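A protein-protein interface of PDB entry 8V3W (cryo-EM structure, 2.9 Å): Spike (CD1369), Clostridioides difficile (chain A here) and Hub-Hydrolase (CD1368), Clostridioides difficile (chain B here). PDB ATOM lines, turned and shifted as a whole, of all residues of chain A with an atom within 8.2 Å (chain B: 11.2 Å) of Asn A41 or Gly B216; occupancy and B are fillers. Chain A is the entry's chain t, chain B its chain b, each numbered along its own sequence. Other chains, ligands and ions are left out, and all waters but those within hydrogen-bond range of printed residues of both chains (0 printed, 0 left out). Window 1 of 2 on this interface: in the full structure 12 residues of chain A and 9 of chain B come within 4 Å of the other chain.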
ATOM      1  N   GLN A  21      30.492  14.923   8.713  1.00  0.00           N
ATOM      2  CA  GLN A  21      30.766  13.535   9.033  1.00  0.00           C
ATOM      3  C   GLN A  21      31.368  13.454  10.427  1.00  0.00           C
ATOM      4  O   GLN A  21      32.052  14.385  10.865  1.00  0.00           O
ATOM      5  CB  GLN A  21      31.733  12.919   8.012  1.00  0.00           C
ATOM      6  CG  GLN A  21      31.060  12.057   6.957  1.00  0.00           C
ATOM      7  CD  GLN A  21      31.067  10.582   7.309  1.00  0.00           C
ATOM      8  OE1 GLN A  21      32.123   9.989   7.531  1.00  0.00           O
ATOM      9  NE2 GLN A  21      29.884   9.982   7.369  1.00  0.00           N
ATOM     10  N   PRO A  22      31.125  12.362  11.148  1.00  0.00           N
ATOM     11  CA  PRO A  22      31.649  12.255  12.514  1.00  0.00           C
ATOM     12  C   PRO A  22      33.169  12.215  12.534  1.00  0.00           C
ATOM     13  O   PRO A  22      33.813  11.749  11.594  1.00  0.00           O
ATOM     14  CB  PRO A  22      31.043  10.943  13.024  1.00  0.00           C
ATOM     15  CG  PRO A  22      30.682  10.188  11.803  1.00  0.00           C
ATOM     16  CD  PRO A  22      30.296  11.204  10.783  1.00  0.00           C
ATOM     17  N   PHE A  24      35.259  10.594  14.771  1.00  0.00           N
ATOM     18  CA  PHE A  24      35.820   9.287  15.064  1.00  0.00           C
ATOM     19  C   PHE A  24      34.697   8.267  15.148  1.00  0.00           C
ATOM     20  O   PHE A  24      33.512   8.605  15.126  1.00  0.00           O
ATOM     21  CB  PHE A  24      36.630   9.306  16.367  1.00  0.00           C
ATOM     22  CG  PHE A  24      35.911   9.950  17.517  1.00  0.00           C
ATOM     23  CD1 PHE A  24      35.018   9.228  18.287  1.00  0.00           C
ATOM     24  CD2 PHE A  24      36.126  11.278  17.825  1.00  0.00           C
ATOM     25  CE1 PHE A  24      34.356   9.819  19.334  1.00  0.00           C
ATOM     26  CE2 PHE A  24      35.468  11.873  18.876  1.00  0.00           C
ATOM     27  CZ  PHE A  24      34.580  11.142  19.630  1.00  0.00           C
ATOM     28  N   PHE A  25      35.088   7.001  15.250  1.00  0.00           N
ATOM     29  CA  PHE A  25      34.156   5.894  15.381  1.00  0.00           C
ATOM     30  C   PHE A  25      34.578   5.020  16.554  1.00  0.00           C
ATOM     31  O   PHE A  25      35.750   4.989  16.929  1.00  0.00           O
ATOM     32  CB  PHE A  25      34.096   5.069  14.096  1.00  0.00           C
ATOM     33  CG  PHE A  25      33.429   5.777  12.957  1.00  0.00           C
ATOM     34  CD1 PHE A  25      34.140   6.646  12.156  1.00  0.00           C
ATOM     35  CD2 PHE A  25      32.090   5.570  12.687  1.00  0.00           C
ATOM     36  CE1 PHE A  25      33.530   7.303  11.109  1.00  0.00           C
ATOM     37  CE2 PHE A  25      31.475   6.222  11.638  1.00  0.00           C
ATOM     38  CZ  PHE A  25      32.198   7.089  10.847  1.00  0.00           C
ATOM     39  N   ILE A  26      33.608   4.328  17.147  1.00  0.00           N
ATOM     40  CA  ILE A  26      33.841   3.405  18.256  1.00  0.00           C
ATOM     41  C   ILE A  26      33.504   1.993  17.779  1.00  0.00           C
ATOM     42  O   ILE A  26      32.427   1.778  17.215  1.00  0.00           O
ATOM     43  CB  ILE A  26      32.995   3.794  19.482  1.00  0.00           C
ATOM     44  CG1 ILE A  26      33.400   5.172  20.007  1.00  0.00           C
ATOM     45  CG2 ILE A  26      33.174   2.783  20.583  1.00  0.00           C
ATOM     46  CD1 ILE A  26      34.796   5.222  20.545  1.00  0.00           C
ATOM     47  N   GLY A  27      34.403   1.039  17.995  1.00  0.00           N
ATOM     48  CA  GLY A  27      34.166  -0.321  17.538  1.00  0.00           C
ATOM     49  C   GLY A  27      34.443  -1.423  18.539  1.00  0.00           C
ATOM     50  O   GLY A  27      35.219  -1.247  19.474  1.00  0.00           O
ATOM     51  N   LYS A  28      33.793  -2.565  18.340  1.00  0.00           N
ATOM     52  CA  LYS A  28      33.968  -3.717  19.218  1.00  0.00           C
ATOM     53  C   LYS A  28      34.533  -4.924  18.467  1.00  0.00           C
ATOM     54  O   LYS A  28      34.022  -5.313  17.419  1.00  0.00           O
ATOM     55  CB  LYS A  28      32.642  -4.084  19.881  1.00  0.00           C
ATOM     56  CG  LYS A  28      32.729  -5.278  20.811  1.00  0.00           C
ATOM     57  CD  LYS A  28      31.405  -5.532  21.507  1.00  0.00           C
ATOM     58  CE  LYS A  28      30.297  -5.786  20.503  1.00  0.00           C
ATOM     59  NZ  LYS A  28      29.004  -6.078  21.181  1.00  0.00           N
ATOM     60  N   ILE A  38      36.401  -6.307  13.465  1.00  0.00           N
ATOM     61  CA  ILE A  38      35.838  -5.184  14.200  1.00  0.00           C
ATOM     62  C   ILE A  38      34.438  -4.868  13.691  1.00  0.00           C
ATOM     63  O   ILE A  38      34.202  -4.833  12.480  1.00  0.00           O
ATOM     64  CB  ILE A  38      36.741  -3.934  14.158  1.00  0.00           C
ATOM     65  CG1 ILE A  38      38.115  -4.265  14.734  1.00  0.00           C
ATOM     66  CG2 ILE A  38      36.129  -2.814  14.969  1.00  0.00           C
ATOM     67  CD1 ILE A  38      39.103  -3.154  14.614  1.00  0.00           C
ATOM     68  N   GLU A  39      33.505  -4.646  14.621  1.00  0.00           N
ATOM     69  CA  GLU A  39      32.116  -4.350  14.290  1.00  0.00           C
ATOM     70  C   GLU A  39      31.768  -2.919  14.673  1.00  0.00           C
ATOM     71  O   GLU A  39      31.948  -2.519  15.828  1.00  0.00           O
ATOM     72  CB  GLU A  39      31.157  -5.309  14.997  1.00  0.00           C
ATOM     73  CG  GLU A  39      29.693  -5.020  14.695  1.00  0.00           C
ATOM     74  CD  GLU A  39      28.800  -5.173  15.907  1.00  0.00           C
ATOM     75  OE1 GLU A  39      29.338  -5.322  17.022  1.00  0.00           O
ATOM     76  OE2 GLU A  39      27.562  -5.141  15.743  1.00  0.00           O
ATOM     77  N   THR A  40      31.259  -2.155  13.710  1.00  0.00           N
ATOM     78  CA  THR A  40      30.773  -0.807  13.973  1.00  0.00           C
ATOM     79  C   THR A  40      29.646  -0.489  13.004  1.00  0.00           C
ATOM     80  O   THR A  40      29.755  -0.789  11.813  1.00  0.00           O
ATOM     81  CB  THR A  40      31.895   0.233  13.844  1.00  0.00           C
ATOM     82  OG1 THR A  40      31.331   1.548  13.848  1.00  0.00           O
ATOM     83  CG2 THR A  40      32.681   0.032  12.560  1.00  0.00           C
ATOM     84  N   ASN A  41      28.572   0.108  13.521  1.00  0.00           N
ATOM     85  CA  ASN A  41      27.428   0.529  12.709  1.00  0.00           C
ATOM     86  C   ASN A  41      26.888  -0.619  11.862  1.00  0.00           C
ATOM     87  O   ASN A  41      26.605  -0.456  10.675  1.00  0.00           O
ATOM     88  CB  ASN A  41      27.789   1.722  11.823  1.00  0.00           C
ATOM     89  CG  ASN A  41      28.305   2.902  12.611  1.00  0.00           C
ATOM     90  OD1 ASN A  41      28.046   3.029  13.803  1.00  0.00           O
ATOM     91  ND2 ASN A  41      29.054   3.769  11.951  1.00  0.00           N
ATOM     92  N   ASN A  42      26.755  -1.794  12.478  1.00  0.00           N
ATOM     93  CA  ASN A  42      26.256  -2.996  11.806  1.00  0.00           C
ATOM     94  C   ASN A  42      27.133  -3.393  10.624  1.00  0.00           C
ATOM     95  O   ASN A  42      26.653  -3.982   9.653  1.00  0.00           O
ATOM     96  CB  ASN A  42      24.805  -2.823  11.351  1.00  0.00           C
ATOM     97  CG  ASN A  42      23.836  -2.758  12.507  1.00  0.00           C
ATOM     98  OD1 ASN A  42      23.845  -3.616  13.387  1.00  0.00           O
ATOM     99  ND2 ASN A  42      22.992  -1.735  12.512  1.00  0.00           N
ATOM    100  N   ILE A  43      28.419  -3.075  10.695  1.00  0.00           N
ATOM    101  CA  ILE A  43      29.381  -3.415   9.657  1.00  0.00           C
ATOM    102  C   ILE A  43      30.547  -4.130  10.320  1.00  0.00           C
ATOM    103  O   ILE A  43      31.049  -3.677  11.352  1.00  0.00           O
ATOM    104  CB  ILE A  43      29.869  -2.167   8.897  1.00  0.00           C
ATOM    105  CG1 ILE A  43      28.805  -1.692   7.910  1.00  0.00           C
ATOM    106  CG2 ILE A  43      31.174  -2.441   8.178  1.00  0.00           C
ATOM    107  CD1 ILE A  43      29.298  -0.642   6.953  1.00  0.00           C
ATOM    108  N   ILE A  44      30.966  -5.248   9.738  1.00  0.00           N
ATOM    109  CA  ILE A  44      32.095  -6.027  10.229  1.00  0.00           C
ATOM    110  C   ILE A  44      33.286  -5.743   9.332  1.00  0.00           C
ATOM    111  O   ILE A  44      33.197  -5.885   8.107  1.00  0.00           O
ATOM    112  CB  ILE A  44      31.778  -7.531  10.252  1.00  0.00           C
ATOM    113  CG1 ILE A  44      30.718  -7.838  11.312  1.00  0.00           C
ATOM    114  CG2 ILE A  44      33.047  -8.340  10.473  1.00  0.00           C
ATOM    115  CD1 ILE A  44      31.280  -8.311  12.629  1.00  0.00           C
ATOM    116  N   LEU A  45      34.397  -5.342   9.936  1.00  0.00           N
ATOM    117  CA  LEU A  45      35.613  -5.061   9.192  1.00  0.00           C
ATOM    118  C   LEU A  45      36.531  -6.277   9.194  1.00  0.00           C
ATOM    119  O   LEU A  45      36.624  -7.012  10.179  1.00  0.00           O
ATOM    120  CB  LEU A  45      36.351  -3.856   9.775  1.00  0.00           C
ATOM    121  CG  LEU A  45      35.510  -2.619  10.069  1.00  0.00           C
ATOM    122  CD1 LEU A  45      36.364  -1.538  10.697  1.00  0.00           C
ATOM    123  CD2 LEU A  45      34.853  -2.115   8.801  1.00  0.00           C
ATOM    124  N   ARG A  94      38.556   7.175  10.255  1.00  0.00           N
ATOM    125  CA  ARG A  94      38.291   6.696   8.905  1.00  0.00           C
ATOM    126  C   ARG A  94      39.151   7.460   7.908  1.00  0.00           C
ATOM    127  O   ARG A  94      39.081   8.690   7.835  1.00  0.00           O
ATOM    128  CB  ARG A  94      36.812   6.845   8.563  1.00  0.00           C
ATOM    129  CG  ARG A  94      36.498   6.609   7.108  1.00  0.00           C
ATOM    130  CD  ARG A  94      35.016   6.723   6.836  1.00  0.00           C
ATOM    131  NE  ARG A  94      34.689   6.300   5.480  1.00  0.00           N
ATOM    132  CZ  ARG A  94      33.460   6.237   4.991  1.00  0.00           C
ATOM    133  NH1 ARG A  94      32.407   6.563   5.723  1.00  0.00           N
ATOM    134  NH2 ARG A  94      33.282   5.842   3.735  1.00  0.00           N
ATOM    135  N   PHE A  99      39.564   1.948   7.913  1.00  0.00           N
ATOM    136  CA  PHE A  99      39.613   2.568   9.225  1.00  0.00           C
ATOM    137  C   PHE A  99      40.974   2.352   9.866  1.00  0.00           C
ATOM    138  O   PHE A  99      41.616   1.318   9.672  1.00  0.00           O
ATOM    139  CB  PHE A  99      38.526   1.993  10.126  1.00  0.00           C
ATOM    140  CG  PHE A  99      37.138   2.396   9.734  1.00  0.00           C
ATOM    141  CD1 PHE A  99      36.501   1.786   8.669  1.00  0.00           C
ATOM    142  CD2 PHE A  99      36.465   3.378  10.434  1.00  0.00           C
ATOM    143  CE1 PHE A  99      35.226   2.152   8.308  1.00  0.00           C
ATOM    144  CE2 PHE A  99      35.190   3.748  10.076  1.00  0.00           C
ATOM    145  CZ  PHE A  99      34.568   3.133   9.012  1.00  0.00           C
ATOM    146  N   ILE B 210      13.876   3.730  16.576  1.00  0.00           N
ATOM    147  CA  ILE B 210      14.939   2.735  16.594  1.00  0.00           C
ATOM    148  C   ILE B 210      16.008   3.194  17.571  1.00  0.00           C
ATOM    149  O   ILE B 210      16.479   4.334  17.491  1.00  0.00           O
ATOM    150  CB  ILE B 210      15.540   2.517  15.196  1.00  0.00           C
ATOM    151  CG1 ILE B 210      14.498   1.912  14.259  1.00  0.00           C
ATOM    152  CG2 ILE B 210      16.763   1.626  15.276  1.00  0.00           C
ATOM    153  CD1 ILE B 210      14.857   2.033  12.804  1.00  0.00           C
ATOM    154  N   VAL B 211      16.399   2.308  18.479  1.00  0.00           N
ATOM    155  CA  VAL B 211      17.427   2.590  19.471  1.00  0.00           C
ATOM    156  C   VAL B 211      18.699   1.864  19.069  1.00  0.00           C
ATOM    157  O   VAL B 211      18.659   0.698  18.662  1.00  0.00           O
ATOM    158  CB  VAL B 211      16.984   2.172  20.885  1.00  0.00           C
ATOM    159  CG1 VAL B 211      17.852   2.845  21.927  1.00  0.00           C
ATOM    160  CG2 VAL B 211      15.523   2.507  21.100  1.00  0.00           C
ATOM    161  N   VAL B 212      19.829   2.557  19.179  1.00  0.00           N
ATOM    162  CA  VAL B 212      21.131   1.984  18.885  1.00  0.00           C
ATOM    163  C   VAL B 212      21.999   2.134  20.124  1.00  0.00           C
ATOM    164  O   VAL B 212      21.815   3.044  20.934  1.00  0.00           O
ATOM    165  CB  VAL B 212      21.809   2.648  17.665  1.00  0.00           C
ATOM    166  CG1 VAL B 212      21.097   2.263  16.385  1.00  0.00           C
ATOM    167  CG2 VAL B 212      21.829   4.153  17.822  1.00  0.00           C
ATOM    168  N   ASP B 213      22.984   1.252  20.239  1.00  0.00           N
ATOM    169  CA  ASP B 213      23.937   1.268  21.341  1.00  0.00           C
ATOM    170  C   ASP B 213      25.049   2.261  21.015  1.00  0.00           C
ATOM    171  O   ASP B 213      24.997   2.939  19.992  1.00  0.00           O
ATOM    172  CB  ASP B 213      24.511  -0.127  21.584  1.00  0.00           C
ATOM    173  CG  ASP B 213      25.207  -0.691  20.364  1.00  0.00           C
ATOM    174  OD1 ASP B 213      25.891   0.077  19.660  1.00  0.00           O
ATOM    175  OD2 ASP B 213      25.076  -1.906  20.110  1.00  0.00           O
ATOM    176  N   GLN B 214      26.057   2.346  21.877  1.00  0.00           N
ATOM    177  CA  GLN B 214      27.174   3.271  21.669  1.00  0.00           C
ATOM    178  C   GLN B 214      27.942   2.982  20.376  1.00  0.00           C
ATOM    179  O   GLN B 214      28.394   3.901  19.697  1.00  0.00           O
ATOM    180  CB  GLN B 214      28.122   3.254  22.869  1.00  0.00           C
ATOM    181  CG  GLN B 214      28.499   1.863  23.350  1.00  0.00           C
ATOM    182  CD  GLN B 214      29.475   1.899  24.509  1.00  0.00           C
ATOM    183  OE1 GLN B 214      29.540   0.966  25.309  1.00  0.00           O
ATOM    184  NE2 GLN B 214      30.240   2.980  24.606  1.00  0.00           N
ATOM    185  N   TYR B 215      28.096   1.702  20.055  1.00  0.00           N
ATOM    186  CA  TYR B 215      28.780   1.241  18.847  1.00  0.00           C
ATOM    187  C   TYR B 215      28.072   1.580  17.522  1.00  0.00           C
ATOM    188  O   TYR B 215      28.703   1.606  16.469  1.00  0.00           O
ATOM    189  CB  TYR B 215      29.065  -0.256  18.945  1.00  0.00           C
ATOM    190  CG  TYR B 215      29.766  -0.633  20.226  1.00  0.00           C
ATOM    191  CD1 TYR B 215      31.109  -0.347  20.413  1.00  0.00           C
ATOM    192  CD2 TYR B 215      29.083  -1.265  21.255  1.00  0.00           C
ATOM    193  CE1 TYR B 215      31.754  -0.683  21.586  1.00  0.00           C
ATOM    194  CE2 TYR B 215      29.719  -1.607  22.431  1.00  0.00           C
ATOM    195  CZ  TYR B 215      31.056  -1.313  22.590  1.00  0.00           C
ATOM    196  OH  TYR B 215      31.696  -1.650  23.758  1.00  0.00           O
ATOM    197  N   GLY B 216      26.769   1.838  17.580  1.00  0.00           N
ATOM    198  CA  GLY B 216      25.982   2.144  16.398  1.00  0.00           C
ATOM    199  C   GLY B 216      25.123   0.980  15.949  1.00  0.00           C
ATOM    200  O   GLY B 216      24.352   1.092  15.001  1.00  0.00           O
ATOM    201  N   SER B 217      25.259  -0.141  16.643  1.00  0.00           N
ATOM    202  CA  SER B 217      24.462  -1.333  16.382  1.00  0.00           C
ATOM    203  C   SER B 217      23.074  -1.221  17.006  1.00  0.00           C
ATOM    204  O   SER B 217      22.914  -0.691  18.106  1.00  0.00           O
ATOM    205  CB  SER B 217      25.188  -2.562  16.919  1.00  0.00           C
ATOM    206  OG  SER B 217      26.339  -2.828  16.137  1.00  0.00           O
ATOM    207  N   LYS B 218      22.070  -1.739  16.303  1.00  0.00           N
ATOM    208  CA  LYS B 218      20.682  -1.611  16.731  1.00  0.00           C
ATOM    209  C   LYS B 218      20.339  -2.647  17.797  1.00  0.00           C
ATOM    210  O   LYS B 218      20.764  -3.801  17.718  1.00  0.00           O
ATOM    211  CB  LYS B 218      19.752  -1.765  15.527  1.00  0.00           C
ATOM    212  CG  LYS B 218      18.282  -1.892  15.863  1.00  0.00           C
ATOM    213  CD  LYS B 218      17.455  -2.025  14.598  1.00  0.00           C
ATOM    214  CE  LYS B 218      17.214  -3.474  14.233  1.00  0.00           C
ATOM    215  NZ  LYS B 218      16.226  -3.587  13.126  1.00  0.00           N
ATOM    216  N   ILE B 219      19.554  -2.233  18.795  1.00  0.00           N
ATOM    217  CA  ILE B 219      19.169  -3.101  19.898  1.00  0.00           C
ATOM    218  C   ILE B 219      17.668  -3.361  19.934  1.00  0.00           C
ATOM    219  O   ILE B 219      17.239  -4.485  20.215  1.00  0.00           O
ATOM    220  CB  ILE B 219      19.657  -2.540  21.250  1.00  0.00           C
ATOM    221  CG1 ILE B 219      19.314  -1.060  21.372  1.00  0.00           C
ATOM    222  CG2 ILE B 219      21.148  -2.752  21.404  1.00  0.00           C
ATOM    223  CD1 ILE B 219      19.855  -0.417  22.627  1.00  0.00           C
ATOM    224  N   SER B 220      16.848  -2.351  19.651  1.00  0.00           N
ATOM    225  CA  SER B 220      15.403  -2.517  19.730  1.00  0.00           C
ATOM    226  C   SER B 220      14.716  -1.529  18.798  1.00  0.00           C
ATOM    227  O   SER B 220      15.328  -0.585  18.296  1.00  0.00           O
ATOM    228  CB  SER B 220      14.904  -2.344  21.167  1.00  0.00           C
ATOM    229  OG  SER B 220      15.037  -1.003  21.594  1.00  0.00           O
ATOM    230  N   GLN B 236      10.580   6.594  10.072  1.00  0.00           N
ATOM    231  CA  GLN B 236      11.378   6.129  11.195  1.00  0.00           C
ATOM    232  C   GLN B 236      12.229   7.245  11.785  1.00  0.00           C
ATOM    233  O   GLN B 236      12.525   8.252  11.140  1.00  0.00           O
ATOM    234  CB  GLN B 236      12.272   4.967  10.767  1.00  0.00           C
ATOM    235  CG  GLN B 236      13.486   5.391   9.979  1.00  0.00           C
ATOM    236  CD  GLN B 236      14.493   4.278   9.808  1.00  0.00           C
ATOM    237  OE1 GLN B 236      14.137   3.101   9.776  1.00  0.00           O
ATOM    238  NE2 GLN B 236      15.763   4.644   9.692  1.00  0.00           N
ATOM    239  N   VAL B 238      15.767   7.626  14.585  1.00  0.00           N
ATOM    240  CA  VAL B 238      16.884   6.913  15.193  1.00  0.00           C
ATOM    241  C   VAL B 238      17.404   7.739  16.356  1.00  0.00           C
ATOM    242  O   VAL B 238      17.756   8.913  16.183  1.00  0.00           O
ATOM    243  CB  VAL B 238      18.001   6.635  14.176  1.00  0.00           C
ATOM    244  CG1 VAL B 238      19.280   6.252  14.890  1.00  0.00           C
ATOM    245  CG2 VAL B 238      17.578   5.544  13.211  1.00  0.00           C
ATOM    246  N   ILE B 239      17.455   7.130  17.539  1.00  0.00           N
ATOM    247  CA  ILE B 239      18.033   7.751  18.722  1.00  0.00           C
ATOM    248  C   ILE B 239      19.093   6.816  19.281  1.00  0.00           C
ATOM    249  O   ILE B 239      19.043   5.599  19.084  1.00  0.00           O
ATOM    250  CB  ILE B 239      16.972   8.078  19.796  1.00  0.00           C
ATOM    251  CG1 ILE B 239      16.529   6.811  20.520  1.00  0.00           C
ATOM    252  CG2 ILE B 239      15.782   8.779  19.176  1.00  0.00           C
ATOM    253  CD1 ILE B 239      15.373   7.023  21.452  1.00  0.00           C
ATOM    254  N   GLN B 240      20.070   7.395  19.973  1.00  0.00           N
ATOM    255  CA  GLN B 240      21.196   6.651  20.517  1.00  0.00           C
ATOM    256  C   GLN B 240      21.225   6.808  22.028  1.00  0.00           C
ATOM    257  O   GLN B 240      21.100   7.923  22.540  1.00  0.00           O
ATOM    258  CB  GLN B 240      22.517   7.133  19.919  1.00  0.00           C
ATOM    259  CG  GLN B 240      23.718   6.298  20.325  1.00  0.00           C
ATOM    260  CD  GLN B 240      25.000   6.794  19.698  1.00  0.00           C
ATOM    261  OE1 GLN B 240      25.151   7.985  19.431  1.00  0.00           O
ATOM    262  NE2 GLN B 240      25.931   5.883  19.455  1.00  0.00           N
ATOM    263  N   GLN B 241      21.393   5.697  22.734  1.00  0.00           N
ATOM    264  CA  GLN B 241      21.531   5.704  24.181  1.00  0.00           C
ATOM    265  C   GLN B 241      22.978   5.411  24.554  1.00  0.00           C
ATOM    266  O   GLN B 241      23.635   4.573  23.930  1.00  0.00           O
ATOM    267  CB  GLN B 241      20.589   4.688  24.836  1.00  0.00           C
ATOM    268  CG  GLN B 241      21.031   3.244  24.741  1.00  0.00           C
ATOM    269  CD  GLN B 241      20.250   2.331  25.662  1.00  0.00           C
ATOM    270  OE1 GLN B 241      19.277   2.746  26.291  1.00  0.00           O
ATOM    271  NE2 GLN B 241      20.678   1.079  25.751  1.00  0.00           N
ATOM    272  N   GLN B 242      23.480   6.137  25.542  1.00  0.00           N
ATOM    273  CA  GLN B 242      24.816   5.908  26.066  1.00  0.00           C
ATOM    274  C   GLN B 242      24.742   4.851  27.164  1.00  0.00           C
ATOM    275  O   GLN B 242      23.724   4.175  27.336  1.00  0.00           O
ATOM    276  CB  GLN B 242      25.425   7.219  26.554  1.00  0.00           C
ATOM    277  CG  GLN B 242      25.868   8.142  25.435  1.00  0.00           C
ATOM    278  CD  GLN B 242      26.968   7.537  24.584  1.00  0.00           C
ATOM    279  OE1 GLN B 242      27.813   6.793  25.081  1.00  0.00           O
ATOM    280  NE2 GLN B 242      26.965   7.857  23.296  1.00  0.00           N
ATOM    281  N   GLU B 243      25.826   4.690  27.920  1.00  0.00           N
ATOM    282  CA  GLU B 243      25.860   3.634  28.925  1.00  0.00           C
ATOM    283  C   GLU B 243      24.992   3.973  30.131  1.00  0.00           C
ATOM    284  O   GLU B 243      24.355   3.086  30.713  1.00  0.00           O
ATOM    285  CB  GLU B 243      27.299   3.368  29.360  1.00  0.00           C
ATOM    286  CG  GLU B 243      27.972   2.254  28.581  1.00  0.00           C
ATOM    287  CD  GLU B 243      27.460   0.878  28.958  1.00  0.00           C
ATOM    288  OE1 GLU B 243      26.684   0.770  29.931  1.00  0.00           O
ATOM    289  OE2 GLU B 243      27.830  -0.098  28.275  1.00  0.00           O
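OD1 of Asn A41 lies close to O of Tyr B215 (3.1 Å). OE2 of Glu A39 is in hydrogen-bond range of OG of Ser B217, 2.6 Å away.
Asn A41 touches two residues of chain B. Of the printed residues of chain A, Gly B216 touches Asn A41. Of chain A, only Glu A39 and Asn A42 come within 4 Å of Ser B217. Printed residues of chain B within 4 Å of Gly A27: Tyr B215. Printed residues of chain A within 4 Å of Lys B218: Asn A42. Of the printed residues of chain B, Ile A26 touches Tyr B215. The nearest residue of chain B that does not touch Asn A41 is Ser B217 (4.5 Å). The nearest printed residue of chain A that does not touch Lys B218 is Glu A39 (6.5 Å).
Of the 17 printed residues of chain A, 7 touch a printed residue of chain B. Along chain A the printed residues that touch a printed residue of chain B span positions 26 to 42. Of the 18 printed residues of chain B, 4 touch a printed residue of chain A. Printed residues of chain B that touch a printed residue of chain A: Tyr B215, Gly B216, Ser B217 and Lys B218.
The backbone NH (N) of Tyr B215 sits at hydrogen-bond distance from the side-chain carboxylate (OD1) of Asp B213 (2.8 Å). The side-chain carboxylate of Asp B213 sits at hydrogen-bond distance from the backbone NH of Gly B216, at 2.9 Å. OD1 of Asp B213 sits at hydrogen-bond distance from N of Ser B217 (3.1 Å). O of Lys A28 sits at hydrogen-bond distance from N of Glu A39.
Among the printed residues, merely in contact across the chains: Asn A41 with Gly B216 (3.4 Å), Thr A40 with Tyr B215 (3.7 Å), Ile A26 with Tyr B215 (3.8 Å), Asn A42 with Ser B217 (3.8 Å), Asn A42 with Lys B218 (3.9 Å), Lys A28 with Tyr B215 (3.9 Å) and Gly A27 with Tyr B215 (3.97 Å).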
